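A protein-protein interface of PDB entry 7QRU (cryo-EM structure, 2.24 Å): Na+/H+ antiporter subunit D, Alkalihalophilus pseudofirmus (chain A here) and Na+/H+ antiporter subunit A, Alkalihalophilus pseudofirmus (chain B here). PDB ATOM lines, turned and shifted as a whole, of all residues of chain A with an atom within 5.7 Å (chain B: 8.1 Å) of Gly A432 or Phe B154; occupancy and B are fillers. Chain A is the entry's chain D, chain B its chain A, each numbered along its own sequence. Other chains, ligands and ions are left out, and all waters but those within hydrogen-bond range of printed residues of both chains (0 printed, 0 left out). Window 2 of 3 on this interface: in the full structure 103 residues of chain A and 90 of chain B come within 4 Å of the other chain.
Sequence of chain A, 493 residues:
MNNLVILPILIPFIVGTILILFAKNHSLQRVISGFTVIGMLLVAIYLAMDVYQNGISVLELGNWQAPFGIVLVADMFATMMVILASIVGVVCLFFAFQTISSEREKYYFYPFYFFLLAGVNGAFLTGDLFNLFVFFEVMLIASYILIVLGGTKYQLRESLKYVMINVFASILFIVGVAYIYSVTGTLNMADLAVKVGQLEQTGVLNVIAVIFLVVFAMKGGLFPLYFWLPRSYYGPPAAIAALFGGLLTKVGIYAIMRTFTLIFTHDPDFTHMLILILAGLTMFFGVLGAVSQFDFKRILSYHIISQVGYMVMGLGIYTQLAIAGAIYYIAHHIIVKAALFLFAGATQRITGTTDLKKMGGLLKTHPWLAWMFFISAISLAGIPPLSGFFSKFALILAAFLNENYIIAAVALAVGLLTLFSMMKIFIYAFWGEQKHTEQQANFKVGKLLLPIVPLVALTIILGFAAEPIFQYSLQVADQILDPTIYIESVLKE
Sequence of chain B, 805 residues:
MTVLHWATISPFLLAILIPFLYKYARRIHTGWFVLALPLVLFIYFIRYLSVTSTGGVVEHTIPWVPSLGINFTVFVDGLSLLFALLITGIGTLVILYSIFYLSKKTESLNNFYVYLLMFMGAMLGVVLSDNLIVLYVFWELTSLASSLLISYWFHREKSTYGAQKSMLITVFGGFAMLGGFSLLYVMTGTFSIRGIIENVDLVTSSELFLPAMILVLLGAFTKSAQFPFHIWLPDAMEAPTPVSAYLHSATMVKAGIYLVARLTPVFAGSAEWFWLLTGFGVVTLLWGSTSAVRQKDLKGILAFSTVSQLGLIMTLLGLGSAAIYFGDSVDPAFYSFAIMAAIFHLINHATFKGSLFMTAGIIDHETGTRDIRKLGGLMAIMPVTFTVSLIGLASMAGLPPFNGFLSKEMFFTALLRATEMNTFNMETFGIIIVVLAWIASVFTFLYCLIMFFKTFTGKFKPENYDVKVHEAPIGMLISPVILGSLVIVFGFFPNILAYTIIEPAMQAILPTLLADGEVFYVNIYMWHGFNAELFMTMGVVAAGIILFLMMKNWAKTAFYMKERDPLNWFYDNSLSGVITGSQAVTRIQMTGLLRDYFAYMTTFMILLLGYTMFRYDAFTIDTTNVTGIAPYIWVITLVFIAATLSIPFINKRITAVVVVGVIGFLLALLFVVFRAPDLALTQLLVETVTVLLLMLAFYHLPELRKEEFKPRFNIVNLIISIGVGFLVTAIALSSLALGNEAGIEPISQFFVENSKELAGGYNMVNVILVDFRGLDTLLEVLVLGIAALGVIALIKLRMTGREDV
The backbone NH of Gly A432 is in hydrogen-bond range of the backbone carbonyl oxygen of Phe B154 (3.0 Å).
The backbone NH (N) of Gly A361 is in hydrogen-bond range of the backbone carbonyl oxygen (O) of Trp A431 (3.2 Å).
N of Leu A363 is in hydrogen-bond range of O of Phe A430, at 2.8 Å.
The side-chain hydroxyl (OG) of Ser B151 lies within hydrogen-bond range of the backbone carbonyl oxygen (O) of Leu B148, at 2.8 Å.
The guanidinium group (NE) of Arg B156 sits close to a ring nitrogen (NE2) of His B155 (3.5 Å).
O of Arg B156 lies within hydrogen-bond range of OG1 of Thr B160 (3.5 Å).
OG1 of Thr B160 sits at hydrogen-bond distance from O of Glu B157.
Leu A363 touches Phe B154.
Lys A364 touches Phe B154.
Trp A431 touches Ser B151 (CZ2 to OG, 3.2 Å).
CB of Phe B154 touches CD1 of Trp A431 (3.3 Å).
CE3 of Trp A431 touches CG2 of Thr B160 (3.8 Å).
His B155 touches Gly A432.
His B155 touches Glu A433 (CB to OE2, 3.6 Å).
Gly A432 touches two residues of chain B.
Phe B154 touches four residues of chain A.
Printed residues of chain B within 4 Å of Glu A433: His B155.
Of the printed residues of chain B, Trp A431 touches Ser B151, Phe B154 and Thr B160.
Printed residues of chain A within 4 Å of His B155: Gly A432 and Glu A433.
Ile B150 touches none of the printed residues of chain A.
The nearest residue of chain B that does not touch Gly A432 is Thr B160 (4.6 Å).
Hydrophobic or aromatic side chains of chain A that line the printed part of chain B: Leu A363 and Trp A431.
Of the 19 printed residues of chain B, 4 touch a printed residue of chain A.
Hydrophobic or aromatic side chains of chain B within 4 Å of the printed part of chain A: Phe B154 and His B155.
Among the printed residues, 8 pairs touch across the chains.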
ATOM      1  N   GLY A 360      12.510  -8.160 -35.217  1.00  0.00           N
ATOM      2  CA  GLY A 360      13.474  -7.962 -34.157  1.00  0.00           C
ATOM      3  C   GLY A 360      13.101  -6.734 -33.346  1.00  0.00           C
ATOM      4  O   GLY A 360      12.623  -5.805 -33.889  1.00  0.00           O
ATOM      5  N   GLY A 361      13.389  -6.696 -32.075  1.00  0.00           N
ATOM      6  CA  GLY A 361      13.314  -5.482 -31.282  1.00  0.00           C
ATOM      7  C   GLY A 361      11.936  -5.195 -30.709  1.00  0.00           C
ATOM      8  O   GLY A 361      11.744  -4.133 -30.178  1.00  0.00           O
ATOM      9  N   LEU A 363      10.783  -6.072 -28.070  1.00  0.00           N
ATOM     10  CA  LEU A 363      10.792  -5.768 -26.649  1.00  0.00           C
ATOM     11  C   LEU A 363      10.936  -4.264 -26.397  1.00  0.00           C
ATOM     12  O   LEU A 363      10.316  -3.695 -25.520  1.00  0.00           O
ATOM     13  CB  LEU A 363      11.851  -6.592 -25.897  1.00  0.00           C
ATOM     14  CG  LEU A 363      12.034  -6.173 -24.458  1.00  0.00           C
ATOM     15  CD1 LEU A 363      10.803  -6.446 -23.659  1.00  0.00           C
ATOM     16  CD2 LEU A 363      13.138  -6.939 -23.889  1.00  0.00           C
ATOM     17  N   LYS A 364      11.651  -3.570 -27.224  1.00  0.00           N
ATOM     18  CA  LYS A 364      11.799  -2.145 -27.037  1.00  0.00           C
ATOM     19  C   LYS A 364      10.506  -1.418 -27.378  1.00  0.00           C
ATOM     20  O   LYS A 364      10.186  -0.490 -26.666  1.00  0.00           O
ATOM     21  CB  LYS A 364      12.869  -1.642 -27.965  1.00  0.00           C
ATOM     22  CG  LYS A 364      13.156  -0.179 -27.970  1.00  0.00           C
ATOM     23  CD  LYS A 364      13.907   0.111 -29.296  1.00  0.00           C
ATOM     24  CE  LYS A 364      14.568   1.467 -29.267  1.00  0.00           C
ATOM     25  NZ  LYS A 364      13.578   2.533 -28.965  1.00  0.00           N
ATOM     26  N   ILE A 427      14.640 -14.448 -28.815  1.00  0.00           N
ATOM     27  CA  ILE A 427      15.856 -13.819 -29.283  1.00  0.00           C
ATOM     28  C   ILE A 427      15.639 -13.124 -30.627  1.00  0.00           C
ATOM     29  O   ILE A 427      16.062 -11.970 -30.814  1.00  0.00           O
ATOM     30  CB  ILE A 427      16.949 -14.892 -29.329  1.00  0.00           C
ATOM     31  CG1 ILE A 427      17.345 -15.374 -27.940  1.00  0.00           C
ATOM     32  CG2 ILE A 427      18.129 -14.457 -30.041  1.00  0.00           C
ATOM     33  CD1 ILE A 427      18.036 -16.659 -27.987  1.00  0.00           C
ATOM     34  N   TYR A 428      14.960 -13.781 -31.558  1.00  0.00           N
ATOM     35  CA  TYR A 428      14.833 -13.251 -32.910  1.00  0.00           C
ATOM     36  C   TYR A 428      13.809 -12.125 -33.033  1.00  0.00           C
ATOM     37  O   TYR A 428      14.113 -11.110 -33.637  1.00  0.00           O
ATOM     38  CB  TYR A 428      14.416 -14.343 -33.877  1.00  0.00           C
ATOM     39  CG  TYR A 428      15.497 -15.176 -34.479  1.00  0.00           C
ATOM     40  CD1 TYR A 428      15.973 -16.301 -33.879  1.00  0.00           C
ATOM     41  CD2 TYR A 428      16.062 -14.807 -35.657  1.00  0.00           C
ATOM     42  CE1 TYR A 428      16.975 -17.065 -34.447  1.00  0.00           C
ATOM     43  CE2 TYR A 428      17.024 -15.582 -36.274  1.00  0.00           C
ATOM     44  CZ  TYR A 428      17.500 -16.711 -35.656  1.00  0.00           C
ATOM     45  OH  TYR A 428      18.506 -17.461 -36.215  1.00  0.00           O
ATOM     46  N   PHE A 430      11.836 -10.444 -30.223  1.00  0.00           N
ATOM     47  CA  PHE A 430      11.723  -9.476 -29.159  1.00  0.00           C
ATOM     48  C   PHE A 430      13.066  -8.825 -28.827  1.00  0.00           C
ATOM     49  O   PHE A 430      13.098  -7.625 -28.652  1.00  0.00           O
ATOM     50  CB  PHE A 430      11.056 -10.199 -27.984  1.00  0.00           C
ATOM     51  CG  PHE A 430       9.611 -10.521 -28.312  1.00  0.00           C
ATOM     52  CD1 PHE A 430       8.592  -9.585 -28.220  1.00  0.00           C
ATOM     53  CD2 PHE A 430       9.284 -11.755 -28.755  1.00  0.00           C
ATOM     54  CE1 PHE A 430       7.328  -9.909 -28.661  1.00  0.00           C
ATOM     55  CE2 PHE A 430       7.981 -12.123 -29.038  1.00  0.00           C
ATOM     56  CZ  PHE A 430       7.033 -11.177 -29.089  1.00  0.00           C
ATOM     57  N   TRP A 431      14.175  -9.531 -28.913  1.00  0.00           N
ATOM     58  CA  TRP A 431      15.506  -8.982 -28.670  1.00  0.00           C
ATOM     59  C   TRP A 431      16.092  -8.627 -29.997  1.00  0.00           C
ATOM     60  O   TRP A 431      15.462  -8.858 -31.006  1.00  0.00           O
ATOM     61  CB  TRP A 431      16.414  -9.997 -27.952  1.00  0.00           C
ATOM     62  CG  TRP A 431      16.011 -10.224 -26.530  1.00  0.00           C
ATOM     63  CD1 TRP A 431      15.419  -9.305 -25.676  1.00  0.00           C
ATOM     64  CD2 TRP A 431      16.439 -11.302 -25.701  1.00  0.00           C
ATOM     65  NE1 TRP A 431      15.364  -9.802 -24.425  1.00  0.00           N
ATOM     66  CE2 TRP A 431      16.085 -10.954 -24.382  1.00  0.00           C
ATOM     67  CE3 TRP A 431      17.254 -12.416 -25.917  1.00  0.00           C
ATOM     68  CZ2 TRP A 431      16.301 -11.804 -23.320  1.00  0.00           C
ATOM     69  CZ3 TRP A 431      17.416 -13.297 -24.881  1.00  0.00           C
ATOM     70  CH2 TRP A 431      16.985 -12.970 -23.594  1.00  0.00           C
ATOM     71  N   GLY A 432      17.288  -8.089 -30.027  1.00  0.00           N
ATOM     72  CA  GLY A 432      17.770  -7.635 -31.314  1.00  0.00           C
ATOM     73  C   GLY A 432      17.544  -6.136 -31.502  1.00  0.00           C
ATOM     74  O   GLY A 432      16.732  -5.527 -30.835  1.00  0.00           O
ATOM     75  N   GLU A 433      18.093  -5.612 -32.589  1.00  0.00           N
ATOM     76  CA  GLU A 433      17.702  -4.308 -33.137  1.00  0.00           C
ATOM     77  C   GLU A 433      16.277  -4.288 -33.767  1.00  0.00           C
ATOM     78  O   GLU A 433      15.833  -5.262 -34.332  1.00  0.00           O
ATOM     79  CB  GLU A 433      18.788  -4.042 -34.167  1.00  0.00           C
ATOM     80  CG  GLU A 433      20.018  -3.371 -33.583  1.00  0.00           C
ATOM     81  CD  GLU A 433      19.803  -1.929 -33.149  1.00  0.00           C
ATOM     82  OE1 GLU A 433      18.853  -1.282 -33.651  1.00  0.00           O
ATOM     83  OE2 GLU A 433      20.590  -1.447 -32.286  1.00  0.00           O
ATOM     84  N   GLN A 434      15.562  -3.181 -33.706  1.00  0.00           N
ATOM     85  CA  GLN A 434      14.233  -3.036 -34.296  1.00  0.00           C
ATOM     86  C   GLN A 434      14.187  -3.201 -35.806  1.00  0.00           C
ATOM     87  O   GLN A 434      14.852  -2.452 -36.456  1.00  0.00           O
ATOM     88  CB  GLN A 434      13.734  -1.635 -34.047  1.00  0.00           C
ATOM     89  CG  GLN A 434      12.316  -1.413 -34.494  1.00  0.00           C
ATOM     90  CD  GLN A 434      11.911   0.028 -34.250  1.00  0.00           C
ATOM     91  OE1 GLN A 434      12.215   0.605 -33.204  1.00  0.00           O
ATOM     92  NE2 GLN A 434      11.251   0.643 -35.226  1.00  0.00           N
ATOM     93  N   SER B 108      17.617   1.755 -18.828  1.00  0.00           N
ATOM     94  CA  SER B 108      16.359   1.200 -18.401  1.00  0.00           C
ATOM     95  C   SER B 108      16.531   0.684 -16.990  1.00  0.00           C
ATOM     96  O   SER B 108      16.526  -0.503 -16.795  1.00  0.00           O
ATOM     97  CB  SER B 108      15.910   0.041 -19.306  1.00  0.00           C
ATOM     98  OG  SER B 108      16.464   0.098 -20.672  1.00  0.00           O
ATOM     99  N   ASN B 111      14.040  -2.256 -15.950  1.00  0.00           N
ATOM    100  CA  ASN B 111      14.395  -3.612 -16.322  1.00  0.00           C
ATOM    101  C   ASN B 111      15.529  -4.129 -15.435  1.00  0.00           C
ATOM    102  O   ASN B 111      15.393  -5.226 -14.902  1.00  0.00           O
ATOM    103  CB  ASN B 111      14.804  -3.792 -17.783  1.00  0.00           C
ATOM    104  CG  ASN B 111      13.598  -3.645 -18.652  1.00  0.00           C
ATOM    105  OD1 ASN B 111      13.117  -4.610 -19.234  1.00  0.00           O
ATOM    106  ND2 ASN B 111      13.092  -2.429 -18.708  1.00  0.00           N
ATOM    107  N   TYR B 115      15.171  -7.346 -12.863  1.00  0.00           N
ATOM    108  CA  TYR B 115      15.888  -8.600 -13.073  1.00  0.00           C
ATOM    109  C   TYR B 115      16.768  -8.849 -11.878  1.00  0.00           C
ATOM    110  O   TYR B 115      16.819  -9.914 -11.370  1.00  0.00           O
ATOM    111  CB  TYR B 115      16.792  -8.550 -14.287  1.00  0.00           C
ATOM    112  CG  TYR B 115      16.121  -8.265 -15.575  1.00  0.00           C
ATOM    113  CD1 TYR B 115      14.730  -8.444 -15.768  1.00  0.00           C
ATOM    114  CD2 TYR B 115      16.886  -7.705 -16.580  1.00  0.00           C
ATOM    115  CE1 TYR B 115      14.157  -8.062 -16.983  1.00  0.00           C
ATOM    116  CE2 TYR B 115      16.321  -7.383 -17.809  1.00  0.00           C
ATOM    117  CZ  TYR B 115      14.950  -7.600 -18.012  1.00  0.00           C
ATOM    118  OH  TYR B 115      14.521  -7.232 -19.252  1.00  0.00           O
ATOM    119  N   LEU B 148      18.395 -12.949 -18.070  1.00  0.00           N
ATOM    120  CA  LEU B 148      17.773 -11.683 -18.389  1.00  0.00           C
ATOM    121  C   LEU B 148      18.798 -10.600 -18.134  1.00  0.00           C
ATOM    122  O   LEU B 148      18.860  -9.691 -18.872  1.00  0.00           O
ATOM    123  CB  LEU B 148      16.527 -11.474 -17.521  1.00  0.00           C
ATOM    124  CG  LEU B 148      15.332 -12.361 -17.925  1.00  0.00           C
ATOM    125  CD1 LEU B 148      14.173 -12.197 -16.974  1.00  0.00           C
ATOM    126  CD2 LEU B 148      14.907 -12.022 -19.313  1.00  0.00           C
ATOM    127  N   LEU B 149      19.569 -10.635 -17.039  1.00  0.00           N
ATOM    128  CA  LEU B 149      20.675  -9.684 -16.871  1.00  0.00           C
ATOM    129  C   LEU B 149      21.781  -9.815 -17.879  1.00  0.00           C
ATOM    130  O   LEU B 149      22.246  -8.788 -18.340  1.00  0.00           O
ATOM    131  CB  LEU B 149      21.260  -9.884 -15.504  1.00  0.00           C
ATOM    132  CG  LEU B 149      20.318  -9.413 -14.379  1.00  0.00           C
ATOM    133  CD1 LEU B 149      20.667 -10.113 -13.097  1.00  0.00           C
ATOM    134  CD2 LEU B 149      20.366  -7.919 -14.220  1.00  0.00           C
ATOM    135  N   ILE B 150      22.203 -11.013 -18.323  1.00  0.00           N
ATOM    136  CA  ILE B 150      23.225 -11.044 -19.386  1.00  0.00           C
ATOM    137  C   ILE B 150      22.721 -10.393 -20.651  1.00  0.00           C
ATOM    138  O   ILE B 150      23.435  -9.733 -21.335  1.00  0.00           O
ATOM    139  CB  ILE B 150      23.670 -12.480 -19.630  1.00  0.00           C
ATOM    140  CG1 ILE B 150      24.370 -12.989 -18.374  1.00  0.00           C
ATOM    141  CG2 ILE B 150      24.551 -12.579 -20.807  1.00  0.00           C
ATOM    142  CD1 ILE B 150      24.326 -14.402 -18.303  1.00  0.00           C
ATOM    143  N   SER B 151      21.441 -10.502 -20.910  1.00  0.00           N
ATOM    144  CA  SER B 151      20.873  -9.939 -22.101  1.00  0.00           C
ATOM    145  C   SER B 151      20.483  -8.481 -21.939  1.00  0.00           C
ATOM    146  O   SER B 151      19.828  -7.968 -22.806  1.00  0.00           O
ATOM    147  CB  SER B 151      19.619 -10.742 -22.427  1.00  0.00           C
ATOM    148  OG  SER B 151      18.529 -10.199 -21.653  1.00  0.00           O
ATOM    149  N   TYR B 152      20.834  -7.767 -20.907  1.00  0.00           N
ATOM    150  CA  TYR B 152      20.272  -6.451 -20.646  1.00  0.00           C
ATOM    151  C   TYR B 152      20.462  -5.515 -21.843  1.00  0.00           C
ATOM    152  O   TYR B 152      19.539  -4.724 -22.121  1.00  0.00           O
ATOM    153  CB  TYR B 152      20.993  -5.876 -19.453  1.00  0.00           C
ATOM    154  CG  TYR B 152      20.598  -4.510 -19.042  1.00  0.00           C
ATOM    155  CD1 TYR B 152      19.327  -4.245 -18.480  1.00  0.00           C
ATOM    156  CD2 TYR B 152      21.509  -3.487 -19.242  1.00  0.00           C
ATOM    157  CE1 TYR B 152      18.945  -2.934 -18.209  1.00  0.00           C
ATOM    158  CE2 TYR B 152      21.171  -2.203 -18.880  1.00  0.00           C
ATOM    159  CZ  TYR B 152      19.897  -1.941 -18.379  1.00  0.00           C
ATOM    160  OH  TYR B 152      19.753  -0.671 -18.046  1.00  0.00           O
ATOM    161  N   TRP B 153      21.587  -5.604 -22.552  1.00  0.00           N
ATOM    162  CA  TRP B 153      21.727  -4.791 -23.748  1.00  0.00           C
ATOM    163  C   TRP B 153      21.296  -5.599 -24.921  1.00  0.00           C
ATOM    164  O   TRP B 153      22.170  -5.997 -25.639  1.00  0.00           O
ATOM    165  CB  TRP B 153      23.115  -4.215 -24.079  1.00  0.00           C
ATOM    166  CG  TRP B 153      23.445  -3.127 -23.107  1.00  0.00           C
ATOM    167  CD1 TRP B 153      22.705  -2.050 -22.751  1.00  0.00           C
ATOM    168  CD2 TRP B 153      24.484  -3.184 -22.134  1.00  0.00           C
ATOM    169  NE1 TRP B 153      23.225  -1.414 -21.646  1.00  0.00           N
ATOM    170  CE2 TRP B 153      24.368  -2.044 -21.309  1.00  0.00           C
ATOM    171  CE3 TRP B 153      25.518  -4.075 -21.937  1.00  0.00           C
ATOM    172  CZ2 TRP B 153      25.224  -1.814 -20.248  1.00  0.00           C
ATOM    173  CZ3 TRP B 153      26.437  -3.781 -20.960  1.00  0.00           C
ATOM    174  CH2 TRP B 153      26.274  -2.687 -20.139  1.00  0.00           C
ATOM    175  N   PHE B 154      19.989  -5.842 -25.049  1.00  0.00           N
ATOM    176  CA  PHE B 154      19.463  -6.923 -25.887  1.00  0.00           C
ATOM    177  C   PHE B 154      19.601  -6.630 -27.379  1.00  0.00           C
ATOM    178  O   PHE B 154      19.539  -7.547 -28.196  1.00  0.00           O
ATOM    179  CB  PHE B 154      18.017  -7.234 -25.512  1.00  0.00           C
ATOM    180  CG  PHE B 154      17.067  -6.105 -25.628  1.00  0.00           C
ATOM    181  CD1 PHE B 154      16.597  -5.709 -26.892  1.00  0.00           C
ATOM    182  CD2 PHE B 154      16.688  -5.395 -24.470  1.00  0.00           C
ATOM    183  CE1 PHE B 154      15.643  -4.695 -26.970  1.00  0.00           C
ATOM    184  CE2 PHE B 154      15.772  -4.371 -24.560  1.00  0.00           C
ATOM    185  CZ  PHE B 154      15.228  -4.035 -25.818  1.00  0.00           C
ATOM    186  N   HIS B 155      19.970  -5.404 -27.720  1.00  0.00           N
ATOM    187  CA  HIS B 155      20.210  -5.040 -29.113  1.00  0.00           C
ATOM    188  C   HIS B 155      21.563  -5.524 -29.602  1.00  0.00           C
ATOM    189  O   HIS B 155      21.767  -5.549 -30.832  1.00  0.00           O
ATOM    190  CB  HIS B 155      20.040  -3.504 -29.368  1.00  0.00           C
ATOM    191  CG  HIS B 155      21.044  -2.683 -28.653  1.00  0.00           C
ATOM    192  ND1 HIS B 155      20.971  -2.455 -27.293  1.00  0.00           N
ATOM    193  CD2 HIS B 155      22.248  -2.237 -29.073  1.00  0.00           C
ATOM    194  CE1 HIS B 155      22.110  -1.890 -26.891  1.00  0.00           C
ATOM    195  NE2 HIS B 155      22.911  -1.737 -27.968  1.00  0.00           N
ATOM    196  N   ARG B 156      22.443  -5.970 -28.709  1.00  0.00           N
ATOM    197  CA  ARG B 156      23.768  -6.446 -29.086  1.00  0.00           C
ATOM    198  C   ARG B 156      23.802  -7.981 -29.215  1.00  0.00           C
ATOM    199  O   ARG B 156      23.145  -8.705 -28.492  1.00  0.00           O
ATOM    200  CB  ARG B 156      24.786  -6.093 -28.053  1.00  0.00           C
ATOM    201  CG  ARG B 156      24.824  -4.626 -27.745  1.00  0.00           C
ATOM    202  CD  ARG B 156      25.914  -4.310 -26.687  1.00  0.00           C
ATOM    203  NE  ARG B 156      25.744  -2.899 -26.317  1.00  0.00           N
ATOM    204  CZ  ARG B 156      26.324  -2.270 -25.293  1.00  0.00           C
ATOM    205  NH1 ARG B 156      27.177  -2.899 -24.501  1.00  0.00           N
ATOM    206  NH2 ARG B 156      26.026  -1.001 -25.063  1.00  0.00           N
ATOM    207  N   GLU B 157      24.433  -8.476 -30.257  1.00  0.00           N
ATOM    208  CA  GLU B 157      24.405  -9.880 -30.563  1.00  0.00           C
ATOM    209  C   GLU B 157      25.131 -10.663 -29.471  1.00  0.00           C
ATOM    210  O   GLU B 157      24.711 -11.757 -29.089  1.00  0.00           O
ATOM    211  CB  GLU B 157      25.016 -10.104 -31.947  1.00  0.00           C
ATOM    212  CG  GLU B 157      24.536 -11.371 -32.626  1.00  0.00           C
ATOM    213  CD  GLU B 157      25.123 -12.670 -32.075  1.00  0.00           C
ATOM    214  OE1 GLU B 157      26.365 -12.694 -31.815  1.00  0.00           O
ATOM    215  OE2 GLU B 157      24.354 -13.674 -31.930  1.00  0.00           O
ATOM    216  N   LYS B 158      26.250 -10.162 -28.981  1.00  0.00           N
ATOM    217  CA  LYS B 158      26.966 -10.830 -27.906  1.00  0.00           C
ATOM    218  C   LYS B 158      26.153 -10.998 -26.620  1.00  0.00           C
ATOM    219  O   LYS B 158      26.265 -11.991 -25.940  1.00  0.00           O
ATOM    220  CB  LYS B 158      28.255 -10.061 -27.709  1.00  0.00           C
ATOM    221  CG  LYS B 158      29.320 -10.629 -28.635  1.00  0.00           C
ATOM    222  CD  LYS B 158      30.552  -9.751 -28.743  1.00  0.00           C
ATOM    223  CE  LYS B 158      31.462  -9.892 -27.546  1.00  0.00           C
ATOM    224  NZ  LYS B 158      32.026 -11.268 -27.478  1.00  0.00           N
ATOM    225  N   SER B 159      25.378 -10.010 -26.277  1.00  0.00           N
ATOM    226  CA  SER B 159      24.482 -10.081 -25.168  1.00  0.00           C
ATOM    227  C   SER B 159      23.464 -11.204 -25.322  1.00  0.00           C
ATOM    228  O   SER B 159      23.286 -11.941 -24.365  1.00  0.00           O
ATOM    229  CB  SER B 159      23.865  -8.720 -25.014  1.00  0.00           C
ATOM    230  OG  SER B 159      24.872  -7.868 -24.404  1.00  0.00           O
ATOM    231  N   THR B 160      22.866 -11.347 -26.497  1.00  0.00           N
ATOM    232  CA  THR B 160      21.852 -12.336 -26.693  1.00  0.00           C
ATOM    233  C   THR B 160      22.458 -13.731 -26.841  1.00  0.00           C
ATOM    234  O   THR B 160      21.857 -14.701 -26.384  1.00  0.00           O
ATOM    235  CB  THR B 160      20.905 -11.894 -27.842  1.00  0.00           C
ATOM    236  OG1 THR B 160      21.581 -11.757 -29.062  1.00  0.00           O
ATOM    237  CG2 THR B 160      20.230 -10.598 -27.519  1.00  0.00           C
ATOM    238  N   TYR B 161      23.698 -13.819 -27.344  1.00  0.00           N
ATOM    239  CA  TYR B 161      24.378 -15.076 -27.453  1.00  0.00           C
ATOM    240  C   TYR B 161      24.682 -15.619 -26.047  1.00  0.00           C
ATOM    241  O   TYR B 161      24.455 -16.798 -25.787  1.00  0.00           O
ATOM    242  CB  TYR B 161      25.577 -14.890 -28.347  1.00  0.00           C
ATOM    243  CG  TYR B 161      26.485 -16.094 -28.434  1.00  0.00           C
ATOM    244  CD1 TYR B 161      26.194 -17.134 -29.314  1.00  0.00           C
ATOM    245  CD2 TYR B 161      27.579 -16.244 -27.552  1.00  0.00           C
ATOM    246  CE1 TYR B 161      26.997 -18.269 -29.396  1.00  0.00           C
ATOM    247  CE2 TYR B 161      28.427 -17.330 -27.704  1.00  0.00           C
ATOM    248  CZ  TYR B 161      28.093 -18.386 -28.572  1.00  0.00           C
ATOM    249  OH  TYR B 161      28.858 -19.501 -28.705  1.00  0.00           O
ATOM    250  N   ALA B 163      23.148 -14.774 -23.245  1.00  0.00           N
ATOM    251  CA  ALA B 163      21.946 -15.046 -22.474  1.00  0.00           C
ATOM    252  C   ALA B 163      21.426 -16.415 -22.897  1.00  0.00           C
ATOM    253  O   ALA B 163      21.160 -17.251 -22.081  1.00  0.00           O
ATOM    254  CB  ALA B 163      20.912 -14.023 -22.763  1.00  0.00           C
ATOM    255  N   GLU B 238      29.196  -9.927 -21.158  1.00  0.00           N
ATOM    256  CA  GLU B 238      28.417  -8.922 -21.866  1.00  0.00           C
ATOM    257  C   GLU B 238      27.464  -8.160 -20.941  1.00  0.00           C
ATOM    258  O   GLU B 238      26.991  -7.109 -21.283  1.00  0.00           O
ATOM    259  CB  GLU B 238      27.711  -9.625 -23.034  1.00  0.00           C
ATOM    260  CG  GLU B 238      28.741 -10.074 -24.070  1.00  0.00           C
ATOM    261  CD  GLU B 238      29.855  -9.062 -24.376  1.00  0.00           C
ATOM    262  OE1 GLU B 238      29.590  -8.052 -25.076  1.00  0.00           O
ATOM    263  OE2 GLU B 238      31.002  -9.288 -23.942  1.00  0.00           O
